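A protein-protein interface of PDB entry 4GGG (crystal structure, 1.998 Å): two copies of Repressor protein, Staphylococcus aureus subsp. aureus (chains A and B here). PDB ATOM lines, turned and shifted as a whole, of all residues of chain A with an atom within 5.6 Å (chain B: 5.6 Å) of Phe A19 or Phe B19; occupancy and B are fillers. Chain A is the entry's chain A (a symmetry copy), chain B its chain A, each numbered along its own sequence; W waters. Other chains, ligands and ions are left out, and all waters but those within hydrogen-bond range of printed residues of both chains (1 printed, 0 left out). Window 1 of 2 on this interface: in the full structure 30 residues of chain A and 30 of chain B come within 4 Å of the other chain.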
ATOM      1  N   ARG A  14      10.642  35.219   8.675  1.00  0.00           N
ATOM      2  CA  ARG A  14       9.329  35.278   8.048  1.00  0.00           C
ATOM      3  C   ARG A  14       9.404  34.799   6.595  1.00  0.00           C
ATOM      4  O   ARG A  14       8.521  34.081   6.134  1.00  0.00           O
ATOM      5  CB  ARG A  14       8.723  36.682   8.155  1.00  0.00           C
ATOM      6  CG  ARG A  14       8.461  37.115   9.596  1.00  0.00           C
ATOM      7  CD  ARG A  14       7.564  38.349   9.689  1.00  0.00           C
ATOM      8  NE  ARG A  14       8.134  39.515   9.019  1.00  0.00           N
ATOM      9  CZ  ARG A  14       9.045  40.322   9.559  1.00  0.00           C
ATOM     10  NH1 ARG A  14       9.502  40.091  10.784  1.00  0.00           N
ATOM     11  NH2 ARG A  14       9.504  41.361   8.872  1.00  0.00           N
ATOM     12  N   VAL A  15      10.461  35.174   5.881  1.00  0.00           N
ATOM     13  CA  VAL A  15      10.635  34.687   4.511  1.00  0.00           C
ATOM     14  C   VAL A  15      10.748  33.166   4.508  1.00  0.00           C
ATOM     15  O   VAL A  15      10.169  32.489   3.653  1.00  0.00           O
ATOM     16  CB  VAL A  15      11.871  35.287   3.819  1.00  0.00           C
ATOM     17  CG1 VAL A  15      12.153  34.562   2.508  1.00  0.00           C
ATOM     18  CG2 VAL A  15      11.681  36.772   3.579  1.00  0.00           C
ATOM     19  N   THR A  16      11.496  32.634   5.470  1.00  0.00           N
ATOM     20  CA  THR A  16      11.624  31.188   5.629  1.00  0.00           C
ATOM     21  C   THR A  16      10.252  30.534   5.781  1.00  0.00           C
ATOM     22  O   THR A  16       9.972  29.512   5.157  1.00  0.00           O
ATOM     23  CB  THR A  16      12.507  30.819   6.849  1.00  0.00           C
ATOM     24  OG1 THR A  16      13.838  31.297   6.639  1.00  0.00           O
ATOM     25  CG2 THR A  16      12.553  29.315   7.037  1.00  0.00           C
ATOM     26  N   GLU A  17       9.396  31.124   6.606  1.00  0.00           N
ATOM     27  CA  GLU A  17       8.057  30.578   6.814  1.00  0.00           C
ATOM     28  C   GLU A  17       7.241  30.618   5.520  1.00  0.00           C
ATOM     29  O   GLU A  17       6.461  29.706   5.236  1.00  0.00           O
ATOM     30  CB  GLU A  17       7.328  31.328   7.933  1.00  0.00           C
ATOM     31  CG  GLU A  17       7.960  31.158   9.310  1.00  0.00           C
ATOM     32  CD  GLU A  17       7.302  32.032  10.368  1.00  0.00           C
ATOM     33  OE1 GLU A  17       7.599  33.247  10.408  1.00  0.00           O
ATOM     34  OE2 GLU A  17       6.489  31.505  11.162  1.00  0.00           O
ATOM     35  N   ILE A  18       7.423  31.671   4.733  1.00  0.00           N
ATOM     36  CA  ILE A  18       6.733  31.773   3.453  1.00  0.00           C
ATOM     37  C   ILE A  18       7.122  30.622   2.528  1.00  0.00           C
ATOM     38  O   ILE A  18       6.254  29.928   1.995  1.00  0.00           O
ATOM     39  CB  ILE A  18       7.017  33.114   2.755  1.00  0.00           C
ATOM     40  CG1 ILE A  18       6.271  34.248   3.462  1.00  0.00           C
ATOM     41  CG2 ILE A  18       6.599  33.052   1.294  1.00  0.00           C
ATOM     42  CD1 ILE A  18       6.650  35.614   2.957  1.00  0.00           C
ATOM     43  N   PHE A  19       8.426  30.420   2.350  1.00  0.00           N
ATOM     44  CA  PHE A  19       8.920  29.341   1.497  1.00  0.00           C
ATOM     45  C   PHE A  19       8.577  27.950   2.007  1.00  0.00           C
ATOM     46  O   PHE A  19       8.280  27.051   1.214  1.00  0.00           O
ATOM     47  CB  PHE A  19      10.425  29.482   1.254  1.00  0.00           C
ATOM     48  CG  PHE A  19      10.768  30.622   0.348  1.00  0.00           C
ATOM     49  CD1 PHE A  19      10.111  30.774  -0.859  1.00  0.00           C
ATOM     50  CD2 PHE A  19      11.713  31.563   0.715  1.00  0.00           C
ATOM     51  CE1 PHE A  19      10.404  31.830  -1.698  1.00  0.00           C
ATOM     52  CE2 PHE A  19      12.011  32.623  -0.121  1.00  0.00           C
ATOM     53  CZ  PHE A  19      11.352  32.756  -1.328  1.00  0.00           C
ATOM     54  N   LYS A  20       8.607  27.765   3.323  1.00  0.00           N
ATOM     55  CA  LYS A  20       8.192  26.489   3.899  1.00  0.00           C
ATOM     56  C   LYS A  20       6.743  26.167   3.540  1.00  0.00           C
ATOM     57  O   LYS A  20       6.402  25.015   3.277  1.00  0.00           O
ATOM     58  CB  LYS A  20       8.382  26.471   5.419  1.00  0.00           C
ATOM     59  CG  LYS A  20       9.818  26.224   5.846  1.00  0.00           C
ATOM     60  CD  LYS A  20       9.959  26.198   7.362  1.00  0.00           C
ATOM     61  CE  LYS A  20      11.392  25.884   7.770  1.00  0.00           C
ATOM     62  NZ  LYS A  20      11.593  25.980   9.244  1.00  0.00           N
ATOM     63  N   ALA A  21       5.896  27.191   3.521  1.00  0.00           N
ATOM     64  CA  ALA A  21       4.487  27.002   3.191  1.00  0.00           C
ATOM     65  C   ALA A  21       4.303  26.555   1.740  1.00  0.00           C
ATOM     66  O   ALA A  21       3.376  25.801   1.427  1.00  0.00           O
ATOM     67  CB  ALA A  21       3.701  28.287   3.458  1.00  0.00           C
ATOM     68  N   LEU A  22       5.189  27.023   0.863  1.00  0.00           N
ATOM     69  CA  LEU A  22       5.106  26.721  -0.566  1.00  0.00           C
ATOM     70  C   LEU A  22       5.734  25.372  -0.929  1.00  0.00           C
ATOM     71  O   LEU A  22       5.587  24.893  -2.053  1.00  0.00           O
ATOM     72  CB  LEU A  22       5.784  27.828  -1.377  1.00  0.00           C
ATOM     73  CG  LEU A  22       5.270  29.261  -1.184  1.00  0.00           C
ATOM     74  CD1 LEU A  22       6.002  30.223  -2.104  1.00  0.00           C
ATOM     75  CD2 LEU A  22       3.775  29.335  -1.415  1.00  0.00           C
ATOM     76  N   GLY A  23       6.438  24.765   0.019  1.00  0.00           N
ATOM     77  CA  GLY A  23       7.206  23.567  -0.260  1.00  0.00           C
ATOM     78  C   GLY A  23       6.366  22.310  -0.290  1.00  0.00           C
ATOM     79  O   GLY A  23       6.643  21.357   0.429  1.00  0.00           O
ATOM     80  N   ILE A  28       1.325  24.007  -4.158  1.00  0.00           N
ATOM     81  CA  ILE A  28       1.733  24.659  -5.398  1.00  0.00           C
ATOM     82  C   ILE A  28       0.617  24.573  -6.447  1.00  0.00           C
ATOM     83  O   ILE A  28       0.340  25.549  -7.147  1.00  0.00           O
ATOM     84  CB  ILE A  28       3.061  24.104  -5.943  1.00  0.00           C
ATOM     85  CG1 ILE A  28       4.214  24.530  -5.029  1.00  0.00           C
ATOM     86  CG2 ILE A  28       3.319  24.617  -7.354  1.00  0.00           C
ATOM     87  CD1 ILE A  28       4.341  26.033  -4.891  1.00  0.00           C
ATOM     88  N   MET A  89       6.410  36.066  -7.404  1.00  0.00           N
ATOM     89  CA  MET A  89       7.244  34.966  -6.922  1.00  0.00           C
ATOM     90  C   MET A  89       6.920  33.650  -7.624  1.00  0.00           C
ATOM     91  O   MET A  89       7.813  32.927  -8.061  1.00  0.00           O
ATOM     92  CB  MET A  89       7.029  34.738  -5.429  1.00  0.00           C
ATOM     93  CG  MET A  89       7.493  35.836  -4.507  1.00  0.00           C
ATOM     94  SD  MET A  89       7.066  35.345  -2.824  1.00  0.00           S
ATOM     95  CE  MET A  89       7.628  33.651  -2.878  1.00  0.00           C
ATOM     96  N   LEU A  90       5.634  33.330  -7.689  1.00  0.00           N
ATOM     97  CA  LEU A  90       5.191  32.067  -8.268  1.00  0.00           C
ATOM     98  C   LEU A  90       5.419  32.014  -9.773  1.00  0.00           C
ATOM     99  O   LEU A  90       5.912  31.015 -10.296  1.00  0.00           O
ATOM    100  CB  LEU A  90       3.712  31.819  -7.963  1.00  0.00           C
ATOM    101  CG  LEU A  90       3.132  30.546  -8.586  1.00  0.00           C
ATOM    102  CD1 LEU A  90       3.880  29.321  -8.083  1.00  0.00           C
ATOM    103  CD2 LEU A  90       1.637  30.414  -8.311  1.00  0.00           C
ATOM    104  N   ALA A  93       9.079  31.704 -10.517  1.00  0.00           N
ATOM    105  CA  ALA A  93       9.536  30.354 -10.170  1.00  0.00           C
ATOM    106  C   ALA A  93       9.123  29.335 -11.232  1.00  0.00           C
ATOM    107  O   ALA A  93       9.922  28.496 -11.652  1.00  0.00           O
ATOM    108  CB  ALA A  93       9.004  29.944  -8.808  1.00  0.00           C
ATOM    109  N   ARG B  14       8.807  20.398 -10.282  1.00  0.00           N
ATOM    110  CA  ARG B  14      10.088  21.089 -10.238  1.00  0.00           C
ATOM    111  C   ARG B  14       9.979  22.374  -9.412  1.00  0.00           C
ATOM    112  O   ARG B  14      10.879  22.692  -8.639  1.00  0.00           O
ATOM    113  CB  ARG B  14      10.623  21.361 -11.648  1.00  0.00           C
ATOM    114  CG  ARG B  14      10.921  20.086 -12.435  1.00  0.00           C
ATOM    115  CD  ARG B  14      11.755  20.345 -13.689  1.00  0.00           C
ATOM    116  NE  ARG B  14      11.097  21.249 -14.629  1.00  0.00           N
ATOM    117  CZ  ARG B  14      10.168  20.876 -15.506  1.00  0.00           C
ATOM    118  NH1 ARG B  14       9.774  19.610 -15.566  1.00  0.00           N
ATOM    119  NH2 ARG B  14       9.627  21.772 -16.324  1.00  0.00           N
ATOM    120  N   VAL B  15       8.875  23.102  -9.555  1.00  0.00           N
ATOM    121  CA  VAL B  15       8.671  24.300  -8.738  1.00  0.00           C
ATOM    122  C   VAL B  15       8.638  23.924  -7.260  1.00  0.00           C
ATOM    123  O   VAL B  15       9.217  24.617  -6.417  1.00  0.00           O
ATOM    124  CB  VAL B  15       7.378  25.051  -9.098  1.00  0.00           C
ATOM    125  CG1 VAL B  15       7.081  26.128  -8.061  1.00  0.00           C
ATOM    126  CG2 VAL B  15       7.479  25.657 -10.484  1.00  0.00           C
ATOM    127  N   THR B  16       7.960  22.823  -6.952  1.00  0.00           N
ATOM    128  CA  THR B  16       7.915  22.308  -5.587  1.00  0.00           C
ATOM    129  C   THR B  16       9.324  22.073  -5.047  1.00  0.00           C
ATOM    130  O   THR B  16       9.632  22.443  -3.915  1.00  0.00           O
ATOM    131  CB  THR B  16       7.103  20.991  -5.495  1.00  0.00           C
ATOM    132  OG1 THR B  16       5.741  21.241  -5.850  1.00  0.00           O
ATOM    133  CG2 THR B  16       7.144  20.438  -4.083  1.00  0.00           C
ATOM    134  N   GLU B  17      10.181  21.464  -5.857  1.00  0.00           N
ATOM    135  CA  GLU B  17      11.555  21.200  -5.435  1.00  0.00           C
ATOM    136  C   GLU B  17      12.313  22.505  -5.187  1.00  0.00           C
ATOM    137  O   GLU B  17      13.128  22.598  -4.266  1.00  0.00           O
ATOM    138  CB  GLU B  17      12.288  20.339  -6.467  1.00  0.00           C
ATOM    139  CG  GLU B  17      11.723  18.931  -6.617  1.00  0.00           C
ATOM    140  CD  GLU B  17      12.377  18.155  -7.751  1.00  0.00           C
ATOM    141  OE1 GLU B  17      12.018  18.399  -8.926  1.00  0.00           O
ATOM    142  OE2 GLU B  17      13.248  17.300  -7.471  1.00  0.00           O
ATOM    143  N   ILE B  18      12.044  23.515  -6.005  1.00  0.00           N
ATOM    144  CA  ILE B  18      12.675  24.816  -5.816  1.00  0.00           C
ATOM    145  C   ILE B  18      12.310  25.409  -4.457  1.00  0.00           C
ATOM    146  O   ILE B  18      13.190  25.801  -3.689  1.00  0.00           O
ATOM    147  CB  ILE B  18      12.292  25.805  -6.930  1.00  0.00           C
ATOM    148  CG1 ILE B  18      13.006  25.438  -8.233  1.00  0.00           C
ATOM    149  CG2 ILE B  18      12.652  27.226  -6.526  1.00  0.00           C
ATOM    150  CD1 ILE B  18      12.535  26.241  -9.415  1.00  0.00           C
ATOM    151  N   PHE B  19      11.012  25.464  -4.164  1.00  0.00           N
ATOM    152  CA  PHE B  19      10.541  25.999  -2.888  1.00  0.00           C
ATOM    153  C   PHE B  19      10.977  25.183  -1.682  1.00  0.00           C
ATOM    154  O   PHE B  19      11.288  25.747  -0.628  1.00  0.00           O
ATOM    155  CB  PHE B  19       9.022  26.190  -2.903  1.00  0.00           C
ATOM    156  CG  PHE B  19       8.583  27.327  -3.769  1.00  0.00           C
ATOM    157  CD1 PHE B  19       9.180  28.568  -3.645  1.00  0.00           C
ATOM    158  CD2 PHE B  19       7.604  27.153  -4.732  1.00  0.00           C
ATOM    159  CE1 PHE B  19       8.798  29.624  -4.448  1.00  0.00           C
ATOM    160  CE2 PHE B  19       7.217  28.206  -5.539  1.00  0.00           C
ATOM    161  CZ  PHE B  19       7.818  29.442  -5.396  1.00  0.00           C
ATOM    162  N   LYS B  20      11.011  23.862  -1.827  1.00  0.00           N
ATOM    163  CA  LYS B  20      11.516  23.014  -0.751  1.00  0.00           C
ATOM    164  C   LYS B  20      12.964  23.359  -0.409  1.00  0.00           C
ATOM    165  O   LYS B  20      13.354  23.349   0.757  1.00  0.00           O
ATOM    166  CB  LYS B  20      11.389  21.528  -1.101  1.00  0.00           C
ATOM    167  CG  LYS B  20       9.988  20.978  -0.909  1.00  0.00           C
ATOM    168  CD  LYS B  20       9.910  19.496  -1.252  1.00  0.00           C
ATOM    169  CE  LYS B  20       8.514  18.949  -0.990  1.00  0.00           C
ATOM    170  NZ  LYS B  20       8.369  17.535  -1.439  1.00  0.00           N
ATOM    171  N   ALA B  21      13.755  23.672  -1.431  1.00  0.00           N
ATOM    172  CA  ALA B  21      15.157  24.020  -1.224  1.00  0.00           C
ATOM    173  C   ALA B  21      15.304  25.325  -0.440  1.00  0.00           C
ATOM    174  O   ALA B  21      16.256  25.493   0.328  1.00  0.00           O
ATOM    175  CB  ALA B  21      15.884  24.118  -2.566  1.00  0.00           C
ATOM    176  N   LEU B  22      14.359  26.242  -0.640  1.00  0.00           N
ATOM    177  CA  LEU B  22      14.400  27.555   0.002  1.00  0.00           C
ATOM    178  C   LEU B  22      13.829  27.544   1.423  1.00  0.00           C
ATOM    179  O   LEU B  22      13.955  28.523   2.158  1.00  0.00           O
ATOM    180  CB  LEU B  22      13.632  28.576  -0.842  1.00  0.00           C
ATOM    181  CG  LEU B  22      14.077  28.767  -2.298  1.00  0.00           C
ATOM    182  CD1 LEU B  22      13.258  29.855  -2.972  1.00  0.00           C
ATOM    183  CD2 LEU B  22      15.555  29.088  -2.374  1.00  0.00           C
ATOM    184  N   GLY B  23      13.198  26.441   1.805  1.00  0.00           N
ATOM    185  CA  GLY B  23      12.483  26.377   3.066  1.00  0.00           C
ATOM    186  C   GLY B  23      13.386  26.143   4.256  1.00  0.00           C
ATOM    187  O   GLY B  23      13.190  25.199   5.012  1.00  0.00           O
ATOM    188  N   ILE B  28      18.168  30.569   3.361  1.00  0.00           N
ATOM    189  CA  ILE B  28      17.676  31.907   3.053  1.00  0.00           C
ATOM    190  C   ILE B  28      18.751  32.960   3.351  1.00  0.00           C
ATOM    191  O   ILE B  28      18.947  33.891   2.567  1.00  0.00           O
ATOM    192  CB  ILE B  28      16.357  32.229   3.780  1.00  0.00           C
ATOM    193  CG1 ILE B  28      15.222  31.387   3.189  1.00  0.00           C
ATOM    194  CG2 ILE B  28      16.016  33.707   3.643  1.00  0.00           C
ATOM    195  CD1 ILE B  28      15.022  31.615   1.705  1.00  0.00           C
ATOM    196  N   MET B  89      12.325  36.395  -7.303  1.00  0.00           N
ATOM    197  CA  MET B  89      11.571  35.616  -6.323  1.00  0.00           C
ATOM    198  C   MET B  89      11.935  35.990  -4.888  1.00  0.00           C
ATOM    199  O   MET B  89      11.064  36.189  -4.044  1.00  0.00           O
ATOM    200  CB  MET B  89      11.859  34.125  -6.480  1.00  0.00           C
ATOM    201  CG  MET B  89      11.376  33.477  -7.752  1.00  0.00           C
ATOM    202  SD  MET B  89      11.897  31.750  -7.709  1.00  0.00           S
ATOM    203  CE  MET B  89      11.424  31.358  -6.033  1.00  0.00           C
ATOM    204  N   LEU B  90      13.232  36.042  -4.615  1.00  0.00           N
ATOM    205  CA  LEU B  90      13.718  36.317  -3.268  1.00  0.00           C
ATOM    206  C   LEU B  90      13.431  37.749  -2.836  1.00  0.00           C
ATOM    207  O   LEU B  90      12.971  37.984  -1.719  1.00  0.00           O
ATOM    208  CB  LEU B  90      15.219  36.038  -3.163  1.00  0.00           C
ATOM    209  CG  LEU B  90      15.838  36.361  -1.801  1.00  0.00           C
ATOM    210  CD1 LEU B  90      15.177  35.535  -0.709  1.00  0.00           C
ATOM    211  CD2 LEU B  90      17.348  36.141  -1.803  1.00  0.00           C
ATOM    212  N   ALA B  93       9.765  38.200  -2.201  1.00  0.00           N
ATOM    213  CA  ALA B  93       9.394  37.509  -0.961  1.00  0.00           C
ATOM    214  C   ALA B  93       9.817  38.310   0.271  1.00  0.00           C
ATOM    215  O   ALA B  93       9.046  38.470   1.220  1.00  0.00           O
ATOM    216  CB  ALA B  93      10.003  36.119  -0.923  1.00  0.00           C
HETATM  217  O   HOH W   1       9.863  24.546   1.734  1.00  0.00           O
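Among the printed residues, pairs that only touch across the chains: Val A15 with Ala B93, Thr A16 with Ile B28, Phe A19 with Phe B19, Phe A19 with Leu B22, Phe A19 with Ile B28, Phe A19 with Ala B93, Lys A20 with Gly B23, Leu A22 with Phe B19, Gly A23 with Lys B20, Ile A28 with Thr B16, Ile A28 with Phe B19, Met A89 with Met B89, Met A89 with Ala B93, Ala A93 with Val B15, Ala A93 with Phe B19 and Ala A93 with Met B89.
Phe A19 touches just these residues of chain B: Phe B19 (3.7 Å), Leu B22 (3.7 Å), Ile B28 (3.5 Å) and Ala B93 (3.6 Å). Printed residues of chain A within 4 Å of Phe B19: Phe A19 (3.7 Å), Leu A22 (3.7 Å), Ile A28 (3.5 Å) and Ala A93 (3.6 Å). Printed residues of chain B within 4 Å of Ala A93: Val B15, Phe B19 and Met B89. Printed residues of chain B within 4 Å of Ile A28: Thr B16 and Phe B19. Of the printed residues of chain A, Ile B28 touches Thr A16 and Phe A19. Of the printed residues of chain A, Ala B93 touches Val A15, Phe A19 and Met A89. Printed residues of chain A within 4 Å of Gly B23: Lys A20 (3.4 Å). The nearest residue of chain B that does not touch Phe A19 is Gly B23 (4.1 Å).
Hydrophobic or aromatic side chains of chain B that line the printed part of chain A: Val B15, Phe B19, Leu B22, Ile B28, Met B89 and Ala B93. Hydrophobic or aromatic side chains of chain A within 4 Å of the printed part of chain B: Val A15, Phe A19, Leu A22, Ile A28, Met A89 and Ala A93. Among the printed residues, 16 pairs touch across the chains. Among the printed residues, no Asp or Glu carboxylate lies within 4 Å of a Lys or Arg side-chain nitrogen of the other chain.
Val A15 touches Ala B93, and with the chains exchanged Ala A93 touches Val B15. Phe A19 touches Leu B22, and with the chains exchanged Leu A22 touches Phe B19. Phe A19 touches Ala B93, and with the chains exchanged Ala A93 touches Phe B19. Met A89 touches Ala B93, and with the chains exchanged Ala A93 touches Met B89. Of the 16 pairs that touch across the chains among the printed residues, 16 have their exchanged pair printed and touching as well.
Water W1 bridges the backbone carbonyl oxygen of Phe B19 and the backbone carbonyl oxygen of Phe A19.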
